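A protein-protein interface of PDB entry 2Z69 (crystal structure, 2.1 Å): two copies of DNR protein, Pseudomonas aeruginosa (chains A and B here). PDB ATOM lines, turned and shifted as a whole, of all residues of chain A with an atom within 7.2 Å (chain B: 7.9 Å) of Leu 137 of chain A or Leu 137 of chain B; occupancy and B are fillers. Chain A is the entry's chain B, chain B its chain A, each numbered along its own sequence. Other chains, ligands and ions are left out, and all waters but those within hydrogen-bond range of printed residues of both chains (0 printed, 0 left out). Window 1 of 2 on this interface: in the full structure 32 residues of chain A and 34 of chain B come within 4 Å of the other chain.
The side-chain carboxylate (OE2) of Glu 89 of chain B is in hydrogen-bond range of the side-chain hydroxyl (OG) of Ser 152 of chain A (2.6 Å).
The side-chain carboxylate of Glu 89 of chain B is in hydrogen-bond range of the backbone NH of Leu 153 of chain A (2.7 Å).
The side-chain hydroxyl of Ser 138 of chain A is in hydrogen-bond range of the backbone carbonyl oxygen of Phe 93 of chain B, 2.5 Å away.
The side-chain carboxylate (OD2) of Asp 95 of chain A lies within hydrogen-bond range of the side-chain hydroxyl (OG1) of Thr 139 of chain B, 3.2 Å away.
NH1 of Arg 140 of chain B lies within hydrogen-bond range of O of Ser 152 of chain A (2.8 Å).
Of chain B, only Leu 134, Leu 137 and Leu 153 come within 4 Å of Leu 137 of chain A.
Leu 137 of chain B touches just these residues of chain A: Leu 134 (3.7 Å), Leu 137 (3.7 Å), Leu 141 (3.4 Å) and Leu 153 (3.7 Å).
Of the printed residues of chain B, Ser 152 of chain A touches Glu 89, Ala 90 and Arg 140.
Of the printed residues of chain B, Leu 131 of chain A touches Ala 130 (3.8 Å).
Printed residues of chain B within 4 Å of Lys 136 of chain A: Leu 153 (3.6 Å).
The nearest printed residue of chain A that does not touch Leu 141 of chain B is Phe 93 of chain A (4.05 Å).
Ala 90 of chain A touches Leu 153 of chain B, and with the chains exchanged Leu 153 of chain A touches Ala 90 of chain B.
Phe 93 of chain A touches Ser 138 of chain B, and with the chains exchanged Ser 138 of chain A touches Phe 93 of chain B.
Leu 134 of chain A touches Leu 137 of chain B, and with the chains exchanged Leu 137 of chain A touches Leu 134 of chain B.
Leu 137 of chain A touches Leu 153 of chain B, and with the chains exchanged Leu 153 of chain A touches Leu 137 of chain B.
Positions printed for both chains: 90, 93, 94, 95, 131, 132, 133, 134, 135, 136, 137, 138, 139, 140, 141, 142, 152 and 153.
Of the 21 printed residues of chain B, 16 touch a printed residue of chain A.
Hydrophobic or aromatic side chains of chain B within 4 Å of the printed part of chain A: Ala 90, Phe 93, Ala 130, Leu 134, Leu 137, Leu 141, His 142 and Leu 153.
Along chain A the printed residues that touch a printed residue of chain B span positions 90 to 153.
Among the printed residues, 31 pairs touch across the chains.
Among the printed residues, no Asp or Glu carboxylate lies within 4 Å of a Lys or Arg side-chain nitrogen of the other chain.
The backbone carbonyl oxygen (O) of Leu 134 of chain B lies within hydrogen-bond range of the side-chain hydroxyl (OG) of Ser 138 of chain B (2.6 Å).
The backbone carbonyl oxygen of Ala 135 of chain B sits at hydrogen-bond distance from the side-chain hydroxyl of Thr 139 of chain B (2.9 Å).
OG1 of Thr 139 of chain A lies within hydrogen-bond range of O of Ala 135 of chain A.
Ser 152 of chain B touches Ala 90 of chain A (O to CB, 3.8 Å).
Leu 134 of chain B touches Leu 133 of chain A.
Leu 137 of chain B touches Leu 134 of chain A.
Leu 153 of chain B touches Leu 137 of chain A.
Thr 139 of chain A touches Asp 95 of chain B (OG1 to OD1, 3.9 Å).
Arg 140 of chain A touches Leu 153 of chain B.
CD1 of Leu 141 of chain A touches CB of Leu 141 of chain B, 3.5 Å away.
His 142 of chain A touches Asp 95 of chain B (CB to OD2, 3.9 Å).
Leu 153 of chain A touches Ala 90 of chain B.
Lys 136 of chain B touches Leu 153 of chain A.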
ATOM      1  N   ALA A  90     -12.702 -17.373  17.862  1.00  0.00           N
ATOM      2  CA  ALA A  90     -11.725 -17.873  16.914  1.00  0.00           C
ATOM      3  C   ALA A  90     -10.957 -16.761  16.209  1.00  0.00           C
ATOM      4  O   ALA A  90      -9.907 -17.019  15.638  1.00  0.00           O
ATOM      5  CB  ALA A  90     -12.385 -18.799  15.885  1.00  0.00           C
ATOM      6  N   PHE A  93      -7.226 -15.869  16.936  1.00  0.00           N
ATOM      7  CA  PHE A  93      -6.214 -16.869  16.577  1.00  0.00           C
ATOM      8  C   PHE A  93      -6.303 -17.173  15.089  1.00  0.00           C
ATOM      9  O   PHE A  93      -6.104 -18.309  14.646  1.00  0.00           O
ATOM     10  CB  PHE A  93      -6.397 -18.147  17.410  1.00  0.00           C
ATOM     11  CG  PHE A  93      -6.420 -17.909  18.894  1.00  0.00           C
ATOM     12  CD1 PHE A  93      -7.635 -17.824  19.577  1.00  0.00           C
ATOM     13  CD2 PHE A  93      -5.232 -17.748  19.607  1.00  0.00           C
ATOM     14  CE1 PHE A  93      -7.675 -17.598  20.960  1.00  0.00           C
ATOM     15  CE2 PHE A  93      -5.256 -17.513  20.996  1.00  0.00           C
ATOM     16  CZ  PHE A  93      -6.482 -17.434  21.673  1.00  0.00           C
ATOM     17  N   MET A  94      -6.640 -16.135  14.335  1.00  0.00           N
ATOM     18  CA  MET A  94      -6.569 -16.125  12.882  1.00  0.00           C
ATOM     19  C   MET A  94      -5.615 -14.988  12.511  1.00  0.00           C
ATOM     20  O   MET A  94      -5.585 -13.949  13.166  1.00  0.00           O
ATOM     21  CB  MET A  94      -7.965 -15.864  12.304  1.00  0.00           C
ATOM     22  CG  MET A  94      -8.839 -17.104  12.238  1.00  0.00           C
ATOM     23  SD  MET A  94     -10.531 -16.795  11.685  1.00  0.00           S
ATOM     24  CE  MET A  94     -10.278 -15.736  10.265  1.00  0.00           C
ATOM     25  N   ASP A  95      -4.821 -15.157  11.480  1.00  0.00           N
ATOM     26  CA  ASP A  95      -3.937 -14.056  11.106  1.00  0.00           C
ATOM     27  C   ASP A  95      -4.681 -13.155  10.126  1.00  0.00           C
ATOM     28  O   ASP A  95      -4.208 -12.888   9.027  1.00  0.00           O
ATOM     29  CB  ASP A  95      -2.605 -14.567  10.563  1.00  0.00           C
ATOM     30  CG  ASP A  95      -1.665 -15.067  11.673  1.00  0.00           C
ATOM     31  OD1 ASP A  95      -1.990 -14.901  12.875  1.00  0.00           O
ATOM     32  OD2 ASP A  95      -0.588 -15.624  11.341  1.00  0.00           O
ATOM     33  N   LEU A 131      -3.189 -23.481  27.586  1.00  0.00           N
ATOM     34  CA  LEU A 131      -3.176 -24.903  27.224  1.00  0.00           C
ATOM     35  C   LEU A 131      -4.517 -25.423  26.725  1.00  0.00           C
ATOM     36  O   LEU A 131      -4.560 -26.249  25.808  1.00  0.00           O
ATOM     37  CB  LEU A 131      -2.685 -25.766  28.405  1.00  0.00           C
ATOM     38  CG  LEU A 131      -1.252 -25.486  28.884  1.00  0.00           C
ATOM     39  CD1 LEU A 131      -0.784 -26.612  29.793  1.00  0.00           C
ATOM     40  CD2 LEU A 131      -0.256 -25.263  27.713  1.00  0.00           C
ATOM     41  N   ALA A 132      -5.600 -24.978  27.356  1.00  0.00           N
ATOM     42  CA  ALA A 132      -6.951 -25.316  26.911  1.00  0.00           C
ATOM     43  C   ALA A 132      -7.221 -24.839  25.468  1.00  0.00           C
ATOM     44  O   ALA A 132      -7.754 -25.591  24.642  1.00  0.00           O
ATOM     45  CB  ALA A 132      -7.999 -24.742  27.877  1.00  0.00           C
ATOM     46  N   LEU A 133      -6.872 -23.588  25.181  1.00  0.00           N
ATOM     47  CA  LEU A 133      -7.069 -23.002  23.837  1.00  0.00           C
ATOM     48  C   LEU A 133      -6.178 -23.694  22.834  1.00  0.00           C
ATOM     49  O   LEU A 133      -6.555 -23.869  21.695  1.00  0.00           O
ATOM     50  CB  LEU A 133      -6.767 -21.504  23.829  1.00  0.00           C
ATOM     51  CG  LEU A 133      -7.743 -20.675  24.674  1.00  0.00           C
ATOM     52  CD1 LEU A 133      -7.143 -19.309  24.957  1.00  0.00           C
ATOM     53  CD2 LEU A 133      -9.105 -20.556  24.000  1.00  0.00           C
ATOM     54  N   LEU A 134      -5.002 -24.104  23.290  1.00  0.00           N
ATOM     55  CA  LEU A 134      -4.062 -24.854  22.482  1.00  0.00           C
ATOM     56  C   LEU A 134      -4.685 -26.204  22.083  1.00  0.00           C
ATOM     57  O   LEU A 134      -4.568 -26.626  20.931  1.00  0.00           O
ATOM     58  CB  LEU A 134      -2.739 -25.041  23.270  1.00  0.00           C
ATOM     59  CG  LEU A 134      -1.414 -25.247  22.541  1.00  0.00           C
ATOM     60  CD1 LEU A 134      -1.298 -24.432  21.259  1.00  0.00           C
ATOM     61  CD2 LEU A 134      -0.275 -24.893  23.478  1.00  0.00           C
ATOM     62  N   ALA A 135      -5.344 -26.867  23.034  1.00  0.00           N
ATOM     63  CA  ALA A 135      -6.114 -28.093  22.748  1.00  0.00           C
ATOM     64  C   ALA A 135      -7.276 -27.878  21.766  1.00  0.00           C
ATOM     65  O   ALA A 135      -7.505 -28.715  20.893  1.00  0.00           O
ATOM     66  CB  ALA A 135      -6.613 -28.745  24.037  1.00  0.00           C
ATOM     67  N   LYS A 136      -7.987 -26.756  21.900  1.00  0.00           N
ATOM     68  CA  LYS A 136      -9.098 -26.415  21.019  1.00  0.00           C
ATOM     69  C   LYS A 136      -8.624 -26.135  19.602  1.00  0.00           C
ATOM     70  O   LYS A 136      -9.169 -26.685  18.638  1.00  0.00           O
ATOM     71  CB  LYS A 136      -9.841 -25.193  21.563  1.00  0.00           C
ATOM     72  CG  LYS A 136     -10.773 -25.459  22.741  1.00  0.00           C
ATOM     73  CD  LYS A 136     -12.106 -25.913  22.231  1.00  0.00           C
ATOM     74  CE  LYS A 136     -12.998 -26.360  23.340  1.00  0.00           C
ATOM     75  NZ  LYS A 136     -14.185 -27.004  22.735  1.00  0.00           N
ATOM     76  N   LEU A 137      -7.612 -25.272  19.491  1.00  0.00           N
ATOM     77  CA  LEU A 137      -7.024 -24.901  18.206  1.00  0.00           C
ATOM     78  C   LEU A 137      -6.489 -26.127  17.505  1.00  0.00           C
ATOM     79  O   LEU A 137      -6.576 -26.233  16.287  1.00  0.00           O
ATOM     80  CB  LEU A 137      -5.858 -23.935  18.397  1.00  0.00           C
ATOM     81  CG  LEU A 137      -6.002 -22.419  18.357  1.00  0.00           C
ATOM     82  CD1 LEU A 137      -4.595 -21.835  18.107  1.00  0.00           C
ATOM     83  CD2 LEU A 137      -6.963 -21.962  17.261  1.00  0.00           C
ATOM     84  N   SER A 138      -5.934 -27.041  18.295  1.00  0.00           N
ATOM     85  CA  SER A 138      -5.371 -28.290  17.803  1.00  0.00           C
ATOM     86  C   SER A 138      -6.416 -29.261  17.223  1.00  0.00           C
ATOM     87  O   SER A 138      -6.161 -29.885  16.188  1.00  0.00           O
ATOM     88  CB  SER A 138      -4.540 -28.946  18.905  1.00  0.00           C
ATOM     89  OG  SER A 138      -4.168 -30.262  18.570  1.00  0.00           O
ATOM     90  N   THR A 139      -7.577 -29.384  17.869  1.00  0.00           N
ATOM     91  CA  THR A 139      -8.678 -30.210  17.341  1.00  0.00           C
ATOM     92  C   THR A 139      -9.243 -29.602  16.047  1.00  0.00           C
ATOM     93  O   THR A 139      -9.609 -30.326  15.119  1.00  0.00           O
ATOM     94  CB  THR A 139      -9.810 -30.431  18.393  1.00  0.00           C
ATOM     95  OG1 THR A 139      -9.239 -30.895  19.618  1.00  0.00           O
ATOM     96  CG2 THR A 139     -10.793 -31.480  17.937  1.00  0.00           C
ATOM     97  N   ARG A 140      -9.292 -28.270  15.997  1.00  0.00           N
ATOM     98  CA  ARG A 140      -9.763 -27.535  14.822  1.00  0.00           C
ATOM     99  C   ARG A 140      -8.787 -27.684  13.643  1.00  0.00           C
ATOM    100  O   ARG A 140      -9.176 -27.579  12.479  1.00  0.00           O
ATOM    101  CB  ARG A 140     -10.022 -26.060  15.174  1.00  0.00           C
ATOM    102  CG  ARG A 140     -10.667 -25.242  14.056  1.00  0.00           C
ATOM    103  CD  ARG A 140     -11.770 -24.326  14.572  1.00  0.00           C
ATOM    104  NE  ARG A 140     -13.056 -25.019  14.686  1.00  0.00           N
ATOM    105  CZ  ARG A 140     -13.579 -25.487  15.820  1.00  0.00           C
ATOM    106  NH1 ARG A 140     -12.943 -25.342  16.975  1.00  0.00           N
ATOM    107  NH2 ARG A 140     -14.753 -26.104  15.800  1.00  0.00           N
ATOM    108  N   LEU A 141      -7.525 -27.951  13.960  1.00  0.00           N
ATOM    109  CA  LEU A 141      -6.485 -28.130  12.956  1.00  0.00           C
ATOM    110  C   LEU A 141      -5.987 -29.575  12.956  1.00  0.00           C
ATOM    111  O   LEU A 141      -4.780 -29.833  12.892  1.00  0.00           O
ATOM    112  CB  LEU A 141      -5.328 -27.155  13.218  1.00  0.00           C
ATOM    113  CG  LEU A 141      -5.331 -25.716  12.672  1.00  0.00           C
ATOM    114  CD1 LEU A 141      -6.722 -25.127  12.414  1.00  0.00           C
ATOM    115  CD2 LEU A 141      -4.532 -24.839  13.630  1.00  0.00           C
ATOM    116  N   HIS A 142      -6.937 -30.504  13.055  1.00  0.00           N
ATOM    117  CA  HIS A 142      -6.675 -31.938  12.950  1.00  0.00           C
ATOM    118  C   HIS A 142      -7.818 -32.556  12.158  1.00  0.00           C
ATOM    119  O   HIS A 142      -7.711 -33.682  11.667  1.00  0.00           O
ATOM    120  CB  HIS A 142      -6.551 -32.587  14.322  1.00  0.00           C
ATOM    121  N   SER A 152       5.823 -30.370  11.372  1.00  0.00           N
ATOM    122  CA  SER A 152       6.549 -29.375  12.126  1.00  0.00           C
ATOM    123  C   SER A 152       5.598 -28.220  12.452  1.00  0.00           C
ATOM    124  O   SER A 152       4.454 -28.189  11.971  1.00  0.00           O
ATOM    125  CB  SER A 152       7.746 -28.885  11.321  1.00  0.00           C
ATOM    126  OG  SER A 152       8.753 -28.352  12.159  1.00  0.00           O
ATOM    127  N   LEU A 153       6.065 -27.287  13.284  1.00  0.00           N
ATOM    128  CA  LEU A 153       5.300 -26.092  13.636  1.00  0.00           C
ATOM    129  C   LEU A 153       5.896 -24.871  12.925  1.00  0.00           C
ATOM    130  O   LEU A 153       6.191 -24.910  11.721  1.00  0.00           O
ATOM    131  CB  LEU A 153       5.267 -25.883  15.164  1.00  0.00           C
ATOM    132  CG  LEU A 153       4.176 -26.448  16.084  1.00  0.00           C
ATOM    133  CD1 LEU A 153       3.070 -25.445  16.293  1.00  0.00           C
ATOM    134  CD2 LEU A 153       3.583 -27.751  15.614  1.00  0.00           C
ATOM    135  N   GLU B  89       7.368 -32.328  15.755  1.00  0.00           N
ATOM    136  CA  GLU B  89       6.821 -31.679  16.952  1.00  0.00           C
ATOM    137  C   GLU B  89       5.307 -31.434  16.801  1.00  0.00           C
ATOM    138  O   GLU B  89       4.588 -31.327  17.784  1.00  0.00           O
ATOM    139  CB  GLU B  89       7.578 -30.381  17.330  1.00  0.00           C
ATOM    140  CG  GLU B  89       7.292 -29.202  16.445  1.00  0.00           C
ATOM    141  CD  GLU B  89       8.250 -29.070  15.266  1.00  0.00           C
ATOM    142  OE1 GLU B  89       8.988 -30.017  14.938  1.00  0.00           O
ATOM    143  OE2 GLU B  89       8.263 -27.993  14.658  1.00  0.00           O
ATOM    144  N   ALA B  90       4.827 -31.434  15.575  1.00  0.00           N
ATOM    145  CA  ALA B  90       3.375 -31.318  15.331  1.00  0.00           C
ATOM    146  C   ALA B  90       2.575 -32.506  15.862  1.00  0.00           C
ATOM    147  O   ALA B  90       1.406 -32.341  16.156  1.00  0.00           O
ATOM    148  CB  ALA B  90       3.076 -31.088  13.873  1.00  0.00           C
ATOM    149  N   PHE B  93       0.396 -32.050  19.046  1.00  0.00           N
ATOM    150  CA  PHE B  93      -0.775 -31.175  18.954  1.00  0.00           C
ATOM    151  C   PHE B  93      -1.702 -31.652  17.833  1.00  0.00           C
ATOM    152  O   PHE B  93      -2.235 -30.855  17.051  1.00  0.00           O
ATOM    153  CB  PHE B  93      -0.325 -29.719  18.778  1.00  0.00           C
ATOM    154  CG  PHE B  93       0.754 -29.310  19.756  1.00  0.00           C
ATOM    155  CD1 PHE B  93       2.097 -29.371  19.404  1.00  0.00           C
ATOM    156  CD2 PHE B  93       0.423 -28.903  21.051  1.00  0.00           C
ATOM    157  CE1 PHE B  93       3.103 -29.007  20.346  1.00  0.00           C
ATOM    158  CE2 PHE B  93       1.422 -28.541  21.983  1.00  0.00           C
ATOM    159  CZ  PHE B  93       2.755 -28.613  21.620  1.00  0.00           C
ATOM    160  N   MET B  94      -1.854 -32.973  17.752  1.00  0.00           N
ATOM    161  CA  MET B  94      -2.920 -33.627  16.984  1.00  0.00           C
ATOM    162  C   MET B  94      -3.324 -34.896  17.733  1.00  0.00           C
ATOM    163  O   MET B  94      -2.509 -35.494  18.447  1.00  0.00           O
ATOM    164  CB  MET B  94      -2.502 -33.911  15.537  1.00  0.00           C
ATOM    165  CG  MET B  94      -1.301 -34.847  15.347  1.00  0.00           C
ATOM    166  SD  MET B  94      -0.947 -35.073  13.585  1.00  0.00           S
ATOM    167  CE  MET B  94       0.148 -33.687  13.270  1.00  0.00           C
ATOM    168  N   ASP B  95      -4.577 -35.295  17.574  1.00  0.00           N
ATOM    169  CA  ASP B  95      -5.207 -36.277  18.461  1.00  0.00           C
ATOM    170  C   ASP B  95      -4.833 -37.743  18.191  1.00  0.00           C
ATOM    171  O   ASP B  95      -5.136 -38.622  19.005  1.00  0.00           O
ATOM    172  CB  ASP B  95      -6.733 -36.107  18.428  1.00  0.00           C
ATOM    173  CG  ASP B  95      -7.162 -34.648  18.348  1.00  0.00           C
ATOM    174  OD1 ASP B  95      -6.633 -33.808  19.117  1.00  0.00           O
ATOM    175  OD2 ASP B  95      -8.041 -34.348  17.515  1.00  0.00           O
ATOM    176  N   ALA B 130       3.583 -21.667  25.694  1.00  0.00           N
ATOM    177  CA  ALA B 130       2.180 -21.917  25.328  1.00  0.00           C
ATOM    178  C   ALA B 130       1.635 -20.823  24.376  1.00  0.00           C
ATOM    179  O   ALA B 130       0.887 -21.117  23.445  1.00  0.00           O
ATOM    180  CB  ALA B 130       1.319 -22.001  26.559  1.00  0.00           C
ATOM    181  N   LEU B 131       2.060 -19.580  24.575  1.00  0.00           N
ATOM    182  CA  LEU B 131       1.596 -18.475  23.717  1.00  0.00           C
ATOM    183  C   LEU B 131       2.217 -18.566  22.332  1.00  0.00           C
ATOM    184  O   LEU B 131       1.515 -18.526  21.330  1.00  0.00           O
ATOM    185  CB  LEU B 131       1.946 -17.138  24.341  1.00  0.00           C
ATOM    186  CG  LEU B 131       1.294 -16.813  25.680  1.00  0.00           C
ATOM    187  CD1 LEU B 131       1.767 -15.454  26.176  1.00  0.00           C
ATOM    188  CD2 LEU B 131      -0.222 -16.904  25.614  1.00  0.00           C
ATOM    189  N   ALA B 132       3.544 -18.736  22.306  1.00  0.00           N
ATOM    190  CA  ALA B 132       4.291 -18.879  21.073  1.00  0.00           C
ATOM    191  C   ALA B 132       3.761 -20.037  20.229  1.00  0.00           C
ATOM    192  O   ALA B 132       3.716 -19.924  19.017  1.00  0.00           O
ATOM    193  CB  ALA B 132       5.778 -19.057  21.379  1.00  0.00           C
ATOM    194  N   LEU B 133       3.385 -21.150  20.861  1.00  0.00           N
ATOM    195  CA  LEU B 133       2.775 -22.288  20.135  1.00  0.00           C
ATOM    196  C   LEU B 133       1.384 -21.943  19.610  1.00  0.00           C
ATOM    197  O   LEU B 133       1.000 -22.378  18.518  1.00  0.00           O
ATOM    198  CB  LEU B 133       2.672 -23.527  21.025  1.00  0.00           C
ATOM    199  CG  LEU B 133       4.006 -24.182  21.400  1.00  0.00           C
ATOM    200  CD1 LEU B 133       3.828 -25.263  22.440  1.00  0.00           C
ATOM    201  CD2 LEU B 133       4.698 -24.743  20.176  1.00  0.00           C
ATOM    202  N   LEU B 134       0.637 -21.160  20.385  1.00  0.00           N
ATOM    203  CA  LEU B 134      -0.669 -20.663  19.923  1.00  0.00           C
ATOM    204  C   LEU B 134      -0.562 -19.816  18.650  1.00  0.00           C
ATOM    205  O   LEU B 134      -1.446 -19.873  17.809  1.00  0.00           O
ATOM    206  CB  LEU B 134      -1.394 -19.891  21.024  1.00  0.00           C
ATOM    207  CG  LEU B 134      -2.229 -20.685  22.035  1.00  0.00           C
ATOM    208  CD1 LEU B 134      -2.555 -19.843  23.275  1.00  0.00           C
ATOM    209  CD2 LEU B 134      -3.536 -21.175  21.427  1.00  0.00           C
ATOM    210  N   ALA B 135       0.503 -19.016  18.538  1.00  0.00           N
ATOM    211  CA  ALA B 135       0.735 -18.131  17.367  1.00  0.00           C
ATOM    212  C   ALA B 135       1.153 -18.954  16.156  1.00  0.00           C
ATOM    213  O   ALA B 135       0.823 -18.618  15.010  1.00  0.00           O
ATOM    214  CB  ALA B 135       1.824 -17.087  17.680  1.00  0.00           C
ATOM    215  N   LYS B 136       1.887 -20.036  16.418  1.00  0.00           N
ATOM    216  CA  LYS B 136       2.286 -20.954  15.366  1.00  0.00           C
ATOM    217  C   LYS B 136       1.062 -21.694  14.801  1.00  0.00           C
ATOM    218  O   LYS B 136       0.908 -21.814  13.571  1.00  0.00           O
ATOM    219  CB  LYS B 136       3.322 -21.947  15.884  1.00  0.00           C
ATOM    220  CG  LYS B 136       4.752 -21.446  15.894  1.00  0.00           C
ATOM    221  CD  LYS B 136       5.301 -21.413  14.486  1.00  0.00           C
ATOM    222  CE  LYS B 136       6.745 -20.931  14.452  1.00  0.00           C
ATOM    223  NZ  LYS B 136       7.291 -21.072  13.063  1.00  0.00           N
ATOM    224  N   LEU B 137       0.198 -22.177  15.690  1.00  0.00           N
ATOM    225  CA  LEU B 137      -1.048 -22.803  15.263  1.00  0.00           C
ATOM    226  C   LEU B 137      -1.981 -21.776  14.586  1.00  0.00           C
ATOM    227  O   LEU B 137      -2.574 -22.072  13.550  1.00  0.00           O
ATOM    228  CB  LEU B 137      -1.748 -23.525  16.430  1.00  0.00           C
ATOM    229  CG  LEU B 137      -1.097 -24.802  16.992  1.00  0.00           C
ATOM    230  CD1 LEU B 137      -2.088 -25.576  17.860  1.00  0.00           C
ATOM    231  CD2 LEU B 137      -0.598 -25.707  15.890  1.00  0.00           C
ATOM    232  N   SER B 138      -2.071 -20.564  15.145  1.00  0.00           N
ATOM    233  CA  SER B 138      -2.785 -19.440  14.490  1.00  0.00           C
ATOM    234  C   SER B 138      -2.425 -19.248  13.013  1.00  0.00           C
ATOM    235  O   SER B 138      -3.321 -19.080  12.185  1.00  0.00           O
ATOM    236  CB  SER B 138      -2.561 -18.128  15.249  1.00  0.00           C
ATOM    237  OG  SER B 138      -2.996 -18.244  16.606  1.00  0.00           O
ATOM    238  N   THR B 139      -1.134 -19.268  12.679  1.00  0.00           N
ATOM    239  CA  THR B 139      -0.694 -19.132  11.274  1.00  0.00           C
ATOM    240  C   THR B 139      -1.151 -20.321  10.407  1.00  0.00           C
ATOM    241  O   THR B 139      -1.426 -20.160   9.214  1.00  0.00           O
ATOM    242  CB  THR B 139       0.842 -18.959  11.159  1.00  0.00           C
ATOM    243  OG1 THR B 139       1.289 -18.080  12.190  1.00  0.00           O
ATOM    244  CG2 THR B 139       1.240 -18.363   9.811  1.00  0.00           C
ATOM    245  N   ARG B 140      -1.233 -21.508  11.006  1.00  0.00           N
ATOM    246  CA  ARG B 140      -1.764 -22.683  10.310  1.00  0.00           C
ATOM    247  C   ARG B 140      -3.282 -22.614  10.104  1.00  0.00           C
ATOM    248  O   ARG B 140      -3.775 -22.935   9.019  1.00  0.00           O
ATOM    249  CB  ARG B 140      -1.345 -23.958  11.030  1.00  0.00           C
ATOM    250  CG  ARG B 140       0.109 -24.277  10.783  1.00  0.00           C
ATOM    251  CD  ARG B 140       0.722 -24.989  11.955  1.00  0.00           C
ATOM    252  NE  ARG B 140       0.803 -26.426  11.732  1.00  0.00           N
ATOM    253  CZ  ARG B 140       1.809 -27.020  11.098  1.00  0.00           C
ATOM    254  NH1 ARG B 140       1.814 -28.341  10.951  1.00  0.00           N
ATOM    255  NH2 ARG B 140       2.815 -26.295  10.620  1.00  0.00           N
ATOM    256  N   LEU B 141      -4.012 -22.161  11.126  1.00  0.00           N
ATOM    257  CA  LEU B 141      -5.459 -21.920  11.014  1.00  0.00           C
ATOM    258  C   LEU B 141      -5.800 -20.767  10.055  1.00  0.00           C
ATOM    259  O   LEU B 141      -6.948 -20.636   9.616  1.00  0.00           O
ATOM    260  CB  LEU B 141      -6.079 -21.672  12.397  1.00  0.00           C
ATOM    261  N   HIS B 142      -4.797 -19.941   9.742  1.00  0.00           N
ATOM    262  CA  HIS B 142      -4.922 -18.860   8.754  1.00  0.00           C
ATOM    263  C   HIS B 142      -5.054 -19.423   7.343  1.00  0.00           C
ATOM    264  O   HIS B 142      -5.002 -18.681   6.356  1.00  0.00           O
ATOM    265  CB  HIS B 142      -3.741 -17.890   8.848  1.00  0.00           C
ATOM    266  N   GLN B 143      -5.205 -20.744   7.262  1.00  0.00           N
ATOM    267  CA  GLN B 143      -5.723 -21.397   6.073  1.00  0.00           C
ATOM    268  C   GLN B 143      -7.221 -21.110   6.065  1.00  0.00           C
ATOM    269  O   GLN B 143      -7.623 -19.948   6.133  1.00  0.00           O
ATOM    270  CB  GLN B 143      -5.438 -22.898   6.099  1.00  0.00           C
ATOM    271  N   SER B 152     -16.090 -20.067  16.091  1.00  0.00           N
ATOM    272  CA  SER B 152     -15.966 -20.493  17.468  1.00  0.00           C
ATOM    273  C   SER B 152     -14.819 -21.481  17.603  1.00  0.00           C
ATOM    274  O   SER B 152     -14.338 -22.030  16.609  1.00  0.00           O
ATOM    275  CB  SER B 152     -17.270 -21.133  17.946  1.00  0.00           C
ATOM    276  OG  SER B 152     -18.225 -20.151  18.314  1.00  0.00           O
ATOM    277  N   LEU B 153     -14.373 -21.688  18.836  1.00  0.00           N
ATOM    278  CA  LEU B 153     -13.305 -22.641  19.102  1.00  0.00           C
ATOM    279  C   LEU B 153     -13.820 -23.923  19.766  1.00  0.00           C
ATOM    280  O   LEU B 153     -14.937 -23.972  20.298  1.00  0.00           O
ATOM    281  CB  LEU B 153     -12.203 -21.992  19.942  1.00  0.00           C
ATOM    282  CG  LEU B 153     -11.389 -20.918  19.227  1.00  0.00           C
ATOM    283  CD1 LEU B 153     -10.361 -20.339  20.162  1.00  0.00           C
ATOM    284  CD2 LEU B 153     -10.716 -21.500  18.014  1.00  0.00           C
